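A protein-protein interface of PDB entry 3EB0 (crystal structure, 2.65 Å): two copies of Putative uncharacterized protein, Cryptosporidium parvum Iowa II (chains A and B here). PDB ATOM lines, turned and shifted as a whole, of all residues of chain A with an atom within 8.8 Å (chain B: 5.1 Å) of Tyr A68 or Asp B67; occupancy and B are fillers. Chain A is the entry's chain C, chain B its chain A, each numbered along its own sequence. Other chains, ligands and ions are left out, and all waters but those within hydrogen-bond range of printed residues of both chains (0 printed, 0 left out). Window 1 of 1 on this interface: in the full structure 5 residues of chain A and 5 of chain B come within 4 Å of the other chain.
Asn A48 touches none of the printed residues of chain B. Of the printed residues of chain B, Lys A55 touches Asp B67 (2.9 Å). Printed residues of chain B within 4 Å of Asp A67: Lys B55 (2.9 Å) and Tyr B68 (3.6 Å). Of chain B, only Asp B67 (3.6 Å) and Tyr B68 (2.7 Å) come within 4 Å of Tyr A68. Printed residues of chain A within 4 Å of Lys B55: Asp A67. No residue of chain A comes within 4 Å of Val B66. Of chain A, only Lys A55 (2.9 Å) and Tyr A68 (3.6 Å) come within 4 Å of Asp B67. Of chain A, only Asp A67 (3.6 Å) and Tyr A68 (2.7 Å) come within 4 Å of Tyr B68. The nearest residue of chain A that does not touch Asp B67 is Asp A52 (5.8 Å). The nearest printed residue of chain B that does not touch Asp A67 is Leu B65 (8.5 Å).
OD1 of Asp A67 is in salt-bridge range of NZ of Lys B55 (2.9 Å). NZ of Lys A55 is in salt-bridge range of OD1 of Asp B67, at 2.9 Å. O of Tyr A68 is in hydrogen-bond range of OH of Tyr B68 (2.7 Å).
OH of Tyr B9 lies within hydrogen-bond range of OD2 of Asp B67 (2.6 Å). The side-chain amino group (NZ) of Lys B55 sits at hydrogen-bond distance from the side-chain hydroxyl (OH) of Tyr B68, at 3.1 Å. O of Asp B67 sits at hydrogen-bond distance from N of Ile B116 (2.9 Å). OH of Tyr A9 sits at hydrogen-bond distance from OD2 of Asp A67. The side-chain amino group (NZ) of Lys A55 lies within hydrogen-bond range of the side-chain hydroxyl (OH) of Tyr A68 (3.3 Å). O of Asp A67 is in hydrogen-bond range of N of Ile A116, 2.7 Å away.
Of the 23 printed residues of chain A, 3 touch a printed residue of chain B. Of the 11 printed residues of chain B, 3 touch a printed residue of chain A. Along chain B the printed residues that touch a printed residue of chain A span positions 55 to 68.
Lys A55 touches Asp B67, and with the chains exchanged Asp A67 touches Lys B55. Asp A67 touches Tyr B68, and with the chains exchanged Tyr A68 touches Asp B67. Tyr A68 touches its own counterpart, Tyr B68. Positions printed for both chains: 9, 55, 65, 66, 67, 68, 69, 114, 115 and 116.
Among the printed residues, merely in contact across the chains: Asp A67 with Tyr B68 (3.6 Å) and Tyr A68 with Asp B67 (3.6 Å).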
ATOM      1  N   TYR A   9     -23.517  -0.489  25.140  1.00  0.00           N
ATOM      2  CA  TYR A   9     -24.848  -1.097  25.048  1.00  0.00           C
ATOM      3  C   TYR A   9     -25.249  -1.814  26.342  1.00  0.00           C
ATOM      4  O   TYR A   9     -24.571  -2.737  26.805  1.00  0.00           O
ATOM      5  CB  TYR A   9     -24.972  -2.021  23.817  1.00  0.00           C
ATOM      6  CG  TYR A   9     -24.680  -1.294  22.524  1.00  0.00           C
ATOM      7  CD1 TYR A   9     -25.657  -0.534  21.891  1.00  0.00           C
ATOM      8  CD2 TYR A   9     -23.407  -1.330  21.958  1.00  0.00           C
ATOM      9  CE1 TYR A   9     -25.383   0.151  20.717  1.00  0.00           C
ATOM     10  CE2 TYR A   9     -23.121  -0.653  20.794  1.00  0.00           C
ATOM     11  CZ  TYR A   9     -24.110   0.090  20.177  1.00  0.00           C
ATOM     12  OH  TYR A   9     -23.802   0.778  19.020  1.00  0.00           O
ATOM     13  N   ALA A  36     -31.357  -3.425  17.949  1.00  0.00           N
ATOM     14  CA  ALA A  36     -31.244  -4.890  18.040  1.00  0.00           C
ATOM     15  C   ALA A  36     -29.796  -5.364  17.943  1.00  0.00           C
ATOM     16  O   ALA A  36     -29.071  -4.971  17.030  1.00  0.00           O
ATOM     17  CB  ALA A  36     -32.106  -5.576  16.999  1.00  0.00           C
ATOM     18  N   LEU A  37     -29.392  -6.202  18.902  1.00  0.00           N
ATOM     19  CA  LEU A  37     -28.057  -6.797  18.924  1.00  0.00           C
ATOM     20  C   LEU A  37     -28.108  -8.247  18.476  1.00  0.00           C
ATOM     21  O   LEU A  37     -28.906  -9.024  18.998  1.00  0.00           O
ATOM     22  CB  LEU A  37     -27.428  -6.697  20.326  1.00  0.00           C
ATOM     23  CG  LEU A  37     -26.272  -7.639  20.747  1.00  0.00           C
ATOM     24  CD1 LEU A  37     -25.005  -7.485  19.930  1.00  0.00           C
ATOM     25  CD2 LEU A  37     -25.923  -7.471  22.225  1.00  0.00           C
ATOM     26  N   LYS A  38     -27.268  -8.609  17.508  1.00  0.00           N
ATOM     27  CA  LYS A  38     -27.090 -10.013  17.143  1.00  0.00           C
ATOM     28  C   LYS A  38     -25.670 -10.445  17.453  1.00  0.00           C
ATOM     29  O   LYS A  38     -24.725 -10.002  16.804  1.00  0.00           O
ATOM     30  CB  LYS A  38     -27.385 -10.243  15.669  1.00  0.00           C
ATOM     31  CG  LYS A  38     -27.323 -11.708  15.261  1.00  0.00           C
ATOM     32  CD  LYS A  38     -28.017 -11.932  13.926  1.00  0.00           C
ATOM     33  CE  LYS A  38     -28.003 -13.402  13.538  1.00  0.00           C
ATOM     34  NZ  LYS A  38     -28.746 -13.615  12.267  1.00  0.00           N
ATOM     35  N   LYS A  47     -14.159 -13.613   7.066  1.00  0.00           N
ATOM     36  CA  LYS A  47     -15.216 -12.617   6.949  1.00  0.00           C
ATOM     37  C   LYS A  47     -16.518 -13.185   7.516  1.00  0.00           C
ATOM     38  O   LYS A  47     -16.694 -14.398   7.621  1.00  0.00           O
ATOM     39  CB  LYS A  47     -15.445 -12.240   5.478  1.00  0.00           C
ATOM     40  CG  LYS A  47     -14.214 -11.782   4.720  1.00  0.00           C
ATOM     41  N   ASN A  48     -17.428 -12.294   7.879  1.00  0.00           N
ATOM     42  CA  ASN A  48     -18.784 -12.670   8.142  1.00  0.00           C
ATOM     43  C   ASN A  48     -19.666 -12.220   6.964  1.00  0.00           C
ATOM     44  O   ASN A  48     -19.867 -11.022   6.729  1.00  0.00           O
ATOM     45  CB  ASN A  48     -19.242 -12.078   9.469  1.00  0.00           C
ATOM     46  CG  ASN A  48     -20.658 -12.537   9.874  1.00  0.00           C
ATOM     47  OD1 ASN A  48     -21.673 -11.986   9.411  1.00  0.00           O
ATOM     48  ND2 ASN A  48     -20.725 -13.522  10.765  1.00  0.00           N
ATOM     49  N   LEU A  51     -22.675  -9.830   7.990  1.00  0.00           N
ATOM     50  CA  LEU A  51     -22.236  -8.438   8.142  1.00  0.00           C
ATOM     51  C   LEU A  51     -22.015  -7.778   6.790  1.00  0.00           C
ATOM     52  O   LEU A  51     -22.566  -6.712   6.527  1.00  0.00           O
ATOM     53  CB  LEU A  51     -20.964  -8.340   8.968  1.00  0.00           C
ATOM     54  CG  LEU A  51     -20.471  -6.914   9.246  1.00  0.00           C
ATOM     55  CD1 LEU A  51     -21.404  -6.192  10.183  1.00  0.00           C
ATOM     56  CD2 LEU A  51     -19.095  -6.957   9.845  1.00  0.00           C
ATOM     57  N   ASP A  52     -21.219  -8.432   5.941  1.00  0.00           N
ATOM     58  CA  ASP A  52     -20.973  -7.981   4.558  1.00  0.00           C
ATOM     59  C   ASP A  52     -22.219  -7.635   3.712  1.00  0.00           C
ATOM     60  O   ASP A  52     -22.174  -6.655   2.960  1.00  0.00           O
ATOM     61  CB  ASP A  52     -20.094  -8.973   3.797  1.00  0.00           C
ATOM     62  CG  ASP A  52     -18.667  -9.016   4.315  1.00  0.00           C
ATOM     63  OD1 ASP A  52     -18.200  -8.022   4.918  1.00  0.00           O
ATOM     64  OD2 ASP A  52     -18.001 -10.055   4.099  1.00  0.00           O
ATOM     65  N   MET A  54     -25.453  -6.931   5.200  1.00  0.00           N
ATOM     66  CA  MET A  54     -25.971  -5.815   5.980  1.00  0.00           C
ATOM     67  C   MET A  54     -25.434  -4.499   5.415  1.00  0.00           C
ATOM     68  O   MET A  54     -26.199  -3.620   4.997  1.00  0.00           O
ATOM     69  CB  MET A  54     -25.548  -5.948   7.452  1.00  0.00           C
ATOM     70  CG  MET A  54     -26.433  -6.849   8.316  1.00  0.00           C
ATOM     71  SD  MET A  54     -28.210  -6.662   8.019  1.00  0.00           S
ATOM     72  CE  MET A  54     -28.590  -5.088   8.800  1.00  0.00           C
ATOM     73  N   LYS A  55     -24.102  -4.408   5.374  1.00  0.00           N
ATOM     74  CA  LYS A  55     -23.363  -3.200   5.029  1.00  0.00           C
ATOM     75  C   LYS A  55     -23.887  -2.442   3.803  1.00  0.00           C
ATOM     76  O   LYS A  55     -23.618  -1.244   3.633  1.00  0.00           O
ATOM     77  CB  LYS A  55     -21.880  -3.540   4.835  1.00  0.00           C
ATOM     78  CG  LYS A  55     -21.063  -3.483   6.098  1.00  0.00           C
ATOM     79  CD  LYS A  55     -19.743  -4.235   5.981  1.00  0.00           C
ATOM     80  CE  LYS A  55     -18.908  -4.032   7.265  1.00  0.00           C
ATOM     81  NZ  LYS A  55     -17.512  -4.575   7.135  1.00  0.00           N
ATOM     82  N   LEU A  65     -28.204  -1.381   9.259  1.00  0.00           N
ATOM     83  CA  LEU A  65     -27.042  -1.563  10.115  1.00  0.00           C
ATOM     84  C   LEU A  65     -26.683  -0.235  10.791  1.00  0.00           C
ATOM     85  O   LEU A  65     -26.741   0.829  10.176  1.00  0.00           O
ATOM     86  CB  LEU A  65     -25.866  -2.111   9.289  1.00  0.00           C
ATOM     87  CG  LEU A  65     -24.470  -2.161   9.927  1.00  0.00           C
ATOM     88  CD1 LEU A  65     -24.370  -3.282  10.946  1.00  0.00           C
ATOM     89  CD2 LEU A  65     -23.395  -2.331   8.864  1.00  0.00           C
ATOM     90  N   VAL A  66     -26.326  -0.289  12.064  1.00  0.00           N
ATOM     91  CA  VAL A  66     -26.044   0.928  12.803  1.00  0.00           C
ATOM     92  C   VAL A  66     -24.626   0.921  13.358  1.00  0.00           C
ATOM     93  O   VAL A  66     -23.962   1.955  13.369  1.00  0.00           O
ATOM     94  CB  VAL A  66     -27.047   1.092  13.951  1.00  0.00           C
ATOM     95  CG1 VAL A  66     -26.604   2.198  14.935  1.00  0.00           C
ATOM     96  CG2 VAL A  66     -28.433   1.367  13.406  1.00  0.00           C
ATOM     97  N   ASP A  67     -24.179  -0.242  13.829  1.00  0.00           N
ATOM     98  CA  ASP A  67     -22.902  -0.392  14.517  1.00  0.00           C
ATOM     99  C   ASP A  67     -22.517  -1.871  14.538  1.00  0.00           C
ATOM    100  O   ASP A  67     -23.375  -2.743  14.400  1.00  0.00           O
ATOM    101  CB  ASP A  67     -23.039   0.126  15.954  1.00  0.00           C
ATOM    102  CG  ASP A  67     -21.700   0.533  16.590  1.00  0.00           C
ATOM    103  OD1 ASP A  67     -20.654  -0.006  16.177  1.00  0.00           O
ATOM    104  OD2 ASP A  67     -21.706   1.382  17.519  1.00  0.00           O
ATOM    105  N   TYR A  68     -21.229  -2.151  14.703  1.00  0.00           N
ATOM    106  CA  TYR A  68     -20.748  -3.508  14.923  1.00  0.00           C
ATOM    107  C   TYR A  68     -19.402  -3.475  15.604  1.00  0.00           C
ATOM    108  O   TYR A  68     -18.625  -2.551  15.382  1.00  0.00           O
ATOM    109  CB  TYR A  68     -20.664  -4.317  13.613  1.00  0.00           C
ATOM    110  CG  TYR A  68     -19.692  -3.813  12.545  1.00  0.00           C
ATOM    111  CD1 TYR A  68     -18.380  -4.327  12.445  1.00  0.00           C
ATOM    112  CD2 TYR A  68     -20.093  -2.852  11.612  1.00  0.00           C
ATOM    113  CE1 TYR A  68     -17.500  -3.873  11.458  1.00  0.00           C
ATOM    114  CE2 TYR A  68     -19.212  -2.397  10.623  1.00  0.00           C
ATOM    115  CZ  TYR A  68     -17.933  -2.912  10.551  1.00  0.00           C
ATOM    116  OH  TYR A  68     -17.098  -2.436   9.576  1.00  0.00           O
ATOM    117  N   PHE A  69     -19.130  -4.493  16.421  1.00  0.00           N
ATOM    118  CA  PHE A  69     -17.872  -4.617  17.167  1.00  0.00           C
ATOM    119  C   PHE A  69     -17.580  -6.058  17.640  1.00  0.00           C
ATOM    120  O   PHE A  69     -18.440  -6.950  17.553  1.00  0.00           O
ATOM    121  CB  PHE A  69     -17.861  -3.634  18.337  1.00  0.00           C
ATOM    122  CG  PHE A  69     -18.935  -3.876  19.332  1.00  0.00           C
ATOM    123  CD1 PHE A  69     -18.682  -4.634  20.469  1.00  0.00           C
ATOM    124  CD2 PHE A  69     -20.196  -3.361  19.134  1.00  0.00           C
ATOM    125  CE1 PHE A  69     -19.674  -4.878  21.389  1.00  0.00           C
ATOM    126  CE2 PHE A  69     -21.194  -3.593  20.041  1.00  0.00           C
ATOM    127  CZ  PHE A  69     -20.936  -4.351  21.182  1.00  0.00           C
ATOM    128  N   TYR A  70     -16.369  -6.285  18.142  1.00  0.00           N
ATOM    129  CA  TYR A  70     -15.948  -7.637  18.530  1.00  0.00           C
ATOM    130  C   TYR A  70     -15.816  -7.746  20.050  1.00  0.00           C
ATOM    131  O   TYR A  70     -15.682  -6.732  20.738  1.00  0.00           O
ATOM    132  CB  TYR A  70     -14.665  -8.057  17.783  1.00  0.00           C
ATOM    133  CG  TYR A  70     -14.813  -8.062  16.264  1.00  0.00           C
ATOM    134  CD1 TYR A  70     -14.980  -9.252  15.554  1.00  0.00           C
ATOM    135  CD2 TYR A  70     -14.800  -6.869  15.541  1.00  0.00           C
ATOM    136  CE1 TYR A  70     -15.123  -9.248  14.154  1.00  0.00           C
ATOM    137  CE2 TYR A  70     -14.942  -6.850  14.154  1.00  0.00           C
ATOM    138  CZ  TYR A  70     -15.104  -8.035  13.465  1.00  0.00           C
ATOM    139  OH  TYR A  70     -15.240  -7.989  12.091  1.00  0.00           O
ATOM    140  N   THR A  71     -15.896  -8.968  20.582  1.00  0.00           N
ATOM    141  CA  THR A  71     -16.020  -9.139  22.039  1.00  0.00           C
ATOM    142  C   THR A  71     -15.543 -10.491  22.598  1.00  0.00           C
ATOM    143  O   THR A  71     -15.141 -11.378  21.845  1.00  0.00           O
ATOM    144  CB  THR A  71     -17.471  -8.789  22.505  1.00  0.00           C
ATOM    145  OG1 THR A  71     -17.417  -8.044  23.722  1.00  0.00           O
ATOM    146  CG2 THR A  71     -18.372 -10.026  22.663  1.00  0.00           C
ATOM    147  N   TYR A 112     -16.602 -13.186  19.665  1.00  0.00           N
ATOM    148  CA  TYR A 112     -17.950 -12.940  19.121  1.00  0.00           C
ATOM    149  C   TYR A 112     -18.039 -11.654  18.314  1.00  0.00           C
ATOM    150  O   TYR A 112     -17.420 -10.647  18.664  1.00  0.00           O
ATOM    151  CB  TYR A 112     -19.006 -12.866  20.236  1.00  0.00           C
ATOM    152  CG  TYR A 112     -19.117 -14.084  21.118  1.00  0.00           C
ATOM    153  CD1 TYR A 112     -19.940 -15.160  20.765  1.00  0.00           C
ATOM    154  CD2 TYR A 112     -18.418 -14.154  22.330  1.00  0.00           C
ATOM    155  CE1 TYR A 112     -20.050 -16.281  21.592  1.00  0.00           C
ATOM    156  CE2 TYR A 112     -18.515 -15.269  23.158  1.00  0.00           C
ATOM    157  CZ  TYR A 112     -19.327 -16.327  22.780  1.00  0.00           C
ATOM    158  OH  TYR A 112     -19.414 -17.419  23.599  1.00  0.00           O
ATOM    159  N   LEU A 113     -18.824 -11.694  17.243  1.00  0.00           N
ATOM    160  CA  LEU A 113     -19.145 -10.508  16.468  1.00  0.00           C
ATOM    161  C   LEU A 113     -20.507 -10.008  16.929  1.00  0.00           C
ATOM    162  O   LEU A 113     -21.461 -10.789  17.017  1.00  0.00           O
ATOM    163  CB  LEU A 113     -19.156 -10.818  14.969  1.00  0.00           C
ATOM    164  CG  LEU A 113     -19.598  -9.717  13.991  1.00  0.00           C
ATOM    165  CD1 LEU A 113     -18.569  -8.608  13.876  1.00  0.00           C
ATOM    166  CD2 LEU A 113     -19.895 -10.265  12.592  1.00  0.00           C
ATOM    167  N   ASN A 114     -20.580  -8.708  17.228  1.00  0.00           N
ATOM    168  CA  ASN A 114     -21.796  -8.056  17.727  1.00  0.00           C
ATOM    169  C   ASN A 114     -22.379  -7.064  16.721  1.00  0.00           C
ATOM    170  O   ASN A 114     -21.826  -5.982  16.524  1.00  0.00           O
ATOM    171  CB  ASN A 114     -21.485  -7.308  19.017  1.00  0.00           C
ATOM    172  CG  ASN A 114     -21.021  -8.218  20.120  1.00  0.00           C
ATOM    173  OD1 ASN A 114     -21.797  -8.559  20.997  1.00  0.00           O
ATOM    174  ND2 ASN A 114     -19.754  -8.611  20.089  1.00  0.00           N
ATOM    175  N   VAL A 115     -23.483  -7.420  16.082  1.00  0.00           N
ATOM    176  CA  VAL A 115     -24.087  -6.557  15.077  1.00  0.00           C
ATOM    177  C   VAL A 115     -25.252  -5.744  15.659  1.00  0.00           C
ATOM    178  O   VAL A 115     -26.277  -6.304  16.102  1.00  0.00           O
ATOM    179  CB  VAL A 115     -24.584  -7.378  13.894  1.00  0.00           C
ATOM    180  CG1 VAL A 115     -25.121  -6.466  12.806  1.00  0.00           C
ATOM    181  CG2 VAL A 115     -23.462  -8.275  13.362  1.00  0.00           C
ATOM    182  N   ILE A 116     -25.106  -4.423  15.653  1.00  0.00           N
ATOM    183  CA  ILE A 116     -26.147  -3.554  16.167  1.00  0.00           C
ATOM    184  C   ILE A 116     -26.967  -3.068  14.991  1.00  0.00           C
ATOM    185  O   ILE A 116     -26.416  -2.530  14.040  1.00  0.00           O
ATOM    186  CB  ILE A 116     -25.549  -2.393  17.013  1.00  0.00           C
ATOM    187  CG1 ILE A 116     -25.381  -2.828  18.470  1.00  0.00           C
ATOM    188  CG2 ILE A 116     -26.484  -1.206  17.058  1.00  0.00           C
ATOM    189  CD1 ILE A 116     -24.426  -3.949  18.704  1.00  0.00           C
ATOM    190  N   MET A 117     -28.277  -3.292  15.045  1.00  0.00           N
ATOM    191  CA  MET A 117     -29.184  -2.951  13.930  1.00  0.00           C
ATOM    192  C   MET A 117     -30.421  -2.156  14.354  1.00  0.00           C
ATOM    193  O   MET A 117     -30.802  -2.166  15.533  1.00  0.00           O
ATOM    194  CB  MET A 117     -29.628  -4.218  13.193  1.00  0.00           C
ATOM    195  CG  MET A 117     -28.503  -4.932  12.487  1.00  0.00           C
ATOM    196  SD  MET A 117     -28.831  -6.638  11.931  1.00  0.00           S
ATOM    197  CE  MET A 117     -28.781  -7.536  13.490  1.00  0.00           C
ATOM    198  N   LYS B   8      -9.741  -8.474   1.497  1.00  0.00           N
ATOM    199  CA  LYS B   8     -10.572  -7.577   0.696  1.00  0.00           C
ATOM    200  C   LYS B   8      -9.786  -6.423   0.076  1.00  0.00           C
ATOM    201  O   LYS B   8     -10.119  -5.931  -1.003  1.00  0.00           O
ATOM    202  CB  LYS B   8     -11.716  -7.020   1.537  1.00  0.00           C
ATOM    203  CG  LYS B   8     -13.051  -7.004   0.819  1.00  0.00           C
ATOM    204  CD  LYS B   8     -13.873  -5.789   1.181  1.00  0.00           C
ATOM    205  CE  LYS B   8     -15.248  -5.887   0.550  1.00  0.00           C
ATOM    206  NZ  LYS B   8     -15.628  -4.598  -0.090  1.00  0.00           N
ATOM    207  N   TYR B   9      -8.734  -5.989   0.754  1.00  0.00           N
ATOM    208  CA  TYR B   9      -7.969  -4.858   0.269  1.00  0.00           C
ATOM    209  C   TYR B   9      -6.532  -5.237  -0.002  1.00  0.00           C
ATOM    210  O   TYR B   9      -5.886  -5.887   0.817  1.00  0.00           O
ATOM    211  CB  TYR B   9      -8.043  -3.712   1.265  1.00  0.00           C
ATOM    212  CG  TYR B   9      -9.462  -3.331   1.606  1.00  0.00           C
ATOM    213  CD1 TYR B   9     -10.165  -2.408   0.831  1.00  0.00           C
ATOM    214  CD2 TYR B   9     -10.103  -3.901   2.703  1.00  0.00           C
ATOM    215  CE1 TYR B   9     -11.461  -2.054   1.145  1.00  0.00           C
ATOM    216  CE2 TYR B   9     -11.408  -3.572   3.021  1.00  0.00           C
ATOM    217  CZ  TYR B   9     -12.084  -2.645   2.249  1.00  0.00           C
ATOM    218  OH  TYR B   9     -13.382  -2.323   2.584  1.00  0.00           O
ATOM    219  N   LYS B  55     -17.935   7.757  12.211  1.00  0.00           N
ATOM    220  CA  LYS B  55     -19.215   7.076  12.036  1.00  0.00           C
ATOM    221  C   LYS B  55     -20.410   7.996  11.888  1.00  0.00           C
ATOM    222  O   LYS B  55     -21.515   7.565  11.578  1.00  0.00           O
ATOM    223  CB  LYS B  55     -19.457   6.152  13.219  1.00  0.00           C
ATOM    224  CG  LYS B  55     -18.923   4.747  13.027  1.00  0.00           C
ATOM    225  CD  LYS B  55     -18.948   3.970  14.338  1.00  0.00           C
ATOM    226  CE  LYS B  55     -18.352   2.584  14.155  1.00  0.00           C
ATOM    227  NZ  LYS B  55     -18.512   1.732  15.375  1.00  0.00           N
ATOM    228  N   LEU B  65     -16.572   7.492   6.007  1.00  0.00           N
ATOM    229  CA  LEU B  65     -16.133   6.165   6.449  1.00  0.00           C
ATOM    230  C   LEU B  65     -16.692   5.128   5.494  1.00  0.00           C
ATOM    231  O   LEU B  65     -17.813   5.273   5.013  1.00  0.00           O
ATOM    232  CB  LEU B  65     -16.593   5.862   7.890  1.00  0.00           C
ATOM    233  CG  LEU B  65     -16.302   4.449   8.442  1.00  0.00           C
ATOM    234  CD1 LEU B  65     -14.815   4.224   8.649  1.00  0.00           C
ATOM    235  CD2 LEU B  65     -17.036   4.174   9.719  1.00  0.00           C
ATOM    236  N   VAL B  66     -15.922   4.081   5.217  1.00  0.00           N
ATOM    237  CA  VAL B  66     -16.371   3.068   4.261  1.00  0.00           C
ATOM    238  C   VAL B  66     -16.491   1.652   4.846  1.00  0.00           C
ATOM    239  O   VAL B  66     -17.465   0.940   4.565  1.00  0.00           O
ATOM    240  CB  VAL B  66     -15.458   3.047   3.020  1.00  0.00           C
ATOM    241  CG1 VAL B  66     -15.832   1.870   2.068  1.00  0.00           C
ATOM    242  CG2 VAL B  66     -15.521   4.395   2.297  1.00  0.00           C
ATOM    243  N   ASP B  67     -15.485   1.273   5.642  1.00  0.00           N
ATOM    244  CA  ASP B  67     -15.327  -0.075   6.195  1.00  0.00           C
ATOM    245  C   ASP B  67     -14.371   0.014   7.387  1.00  0.00           C
ATOM    246  O   ASP B  67     -13.629   0.985   7.504  1.00  0.00           O
ATOM    247  CB  ASP B  67     -14.754  -1.003   5.111  1.00  0.00           C
ATOM    248  CG  ASP B  67     -14.937  -2.492   5.419  1.00  0.00           C
ATOM    249  OD1 ASP B  67     -15.204  -2.836   6.590  1.00  0.00           O
ATOM    250  OD2 ASP B  67     -14.805  -3.326   4.480  1.00  0.00           O
ATOM    251  N   TYR B  68     -14.390  -0.973   8.276  1.00  0.00           N
ATOM    252  CA  TYR B  68     -13.377  -1.066   9.328  1.00  0.00           C
ATOM    253  C   TYR B  68     -13.343  -2.463   9.899  1.00  0.00           C
ATOM    254  O   TYR B  68     -14.382  -3.106  10.026  1.00  0.00           O
ATOM    255  CB  TYR B  68     -13.603  -0.039  10.452  1.00  0.00           C
ATOM    256  CG  TYR B  68     -14.888  -0.218  11.266  1.00  0.00           C
ATOM    257  CD1 TYR B  68     -14.922  -1.037  12.403  1.00  0.00           C
ATOM    258  CD2 TYR B  68     -16.064   0.441  10.897  1.00  0.00           C
ATOM    259  CE1 TYR B  68     -16.088  -1.194  13.134  1.00  0.00           C
ATOM    260  CE2 TYR B  68     -17.238   0.282  11.629  1.00  0.00           C
ATOM    261  CZ  TYR B  68     -17.241  -0.527  12.743  1.00  0.00           C
ATOM    262  OH  TYR B  68     -18.405  -0.669  13.461  1.00  0.00           O
ATOM    263  N   PHE B  69     -12.146  -2.915  10.260  1.00  0.00           N
ATOM    264  CA  PHE B  69     -11.929  -4.282  10.745  1.00  0.00           C
ATOM    265  C   PHE B  69     -10.661  -4.388  11.583  1.00  0.00           C
ATOM    266  O   PHE B  69      -9.833  -3.476  11.584  1.00  0.00           O
ATOM    267  CB  PHE B  69     -11.891  -5.285   9.576  1.00  0.00           C
ATOM    268  CG  PHE B  69     -10.807  -5.024   8.558  1.00  0.00           C
ATOM    269  CD1 PHE B  69      -9.578  -5.678   8.645  1.00  0.00           C
ATOM    270  CD2 PHE B  69     -11.020  -4.151   7.494  1.00  0.00           C
ATOM    271  CE1 PHE B  69      -8.568  -5.444   7.699  1.00  0.00           C
ATOM    272  CE2 PHE B  69     -10.018  -3.925   6.542  1.00  0.00           C
ATOM    273  CZ  PHE B  69      -8.794  -4.573   6.648  1.00  0.00           C
ATOM    274  N   ASN B 114      -8.281  -1.188  11.584  1.00  0.00           N
ATOM    275  CA  ASN B 114      -8.140  -0.837  10.183  1.00  0.00           C
ATOM    276  C   ASN B 114      -9.317  -0.029   9.685  1.00  0.00           C
ATOM    277  O   ASN B 114     -10.415  -0.542   9.549  1.00  0.00           O
ATOM    278  CB  ASN B 114      -7.982  -2.101   9.347  1.00  0.00           C
ATOM    279  CG  ASN B 114      -6.726  -2.857   9.678  1.00  0.00           C
ATOM    280  OD1 ASN B 114      -5.695  -2.642   9.049  1.00  0.00           O
ATOM    281  ND2 ASN B 114      -6.796  -3.741  10.669  1.00  0.00           N
ATOM    282  N   VAL B 115      -9.072   1.235   9.404  1.00  0.00           N
ATOM    283  CA  VAL B 115     -10.117   2.152   8.992  1.00  0.00           C
ATOM    284  C   VAL B 115     -10.045   2.428   7.490  1.00  0.00           C
ATOM    285  O   VAL B 115      -9.074   3.004   7.007  1.00  0.00           O
ATOM    286  CB  VAL B 115     -10.034   3.477   9.774  1.00  0.00           C
ATOM    287  CG1 VAL B 115     -11.253   4.319   9.498  1.00  0.00           C
ATOM    288  CG2 VAL B 115      -9.940   3.208  11.273  1.00  0.00           C
ATOM    289  N   ILE B 116     -11.074   2.021   6.759  1.00  0.00           N
ATOM    290  CA  ILE B 116     -11.133   2.245   5.318  1.00  0.00           C
ATOM    291  C   ILE B 116     -11.967   3.498   5.037  1.00  0.00           C
ATOM    292  O   ILE B 116     -13.118   3.591   5.478  1.00  0.00           O
ATOM    293  CB  ILE B 116     -11.651   0.955   4.561  1.00  0.00           C
ATOM    294  CG1 ILE B 116     -10.486   0.070   4.123  1.00  0.00           C
ATOM    295  CG2 ILE B 116     -12.353   1.291   3.275  1.00  0.00           C
ATOM    296  CD1 ILE B 116      -9.636  -0.434   5.238  1.00  0.00           C
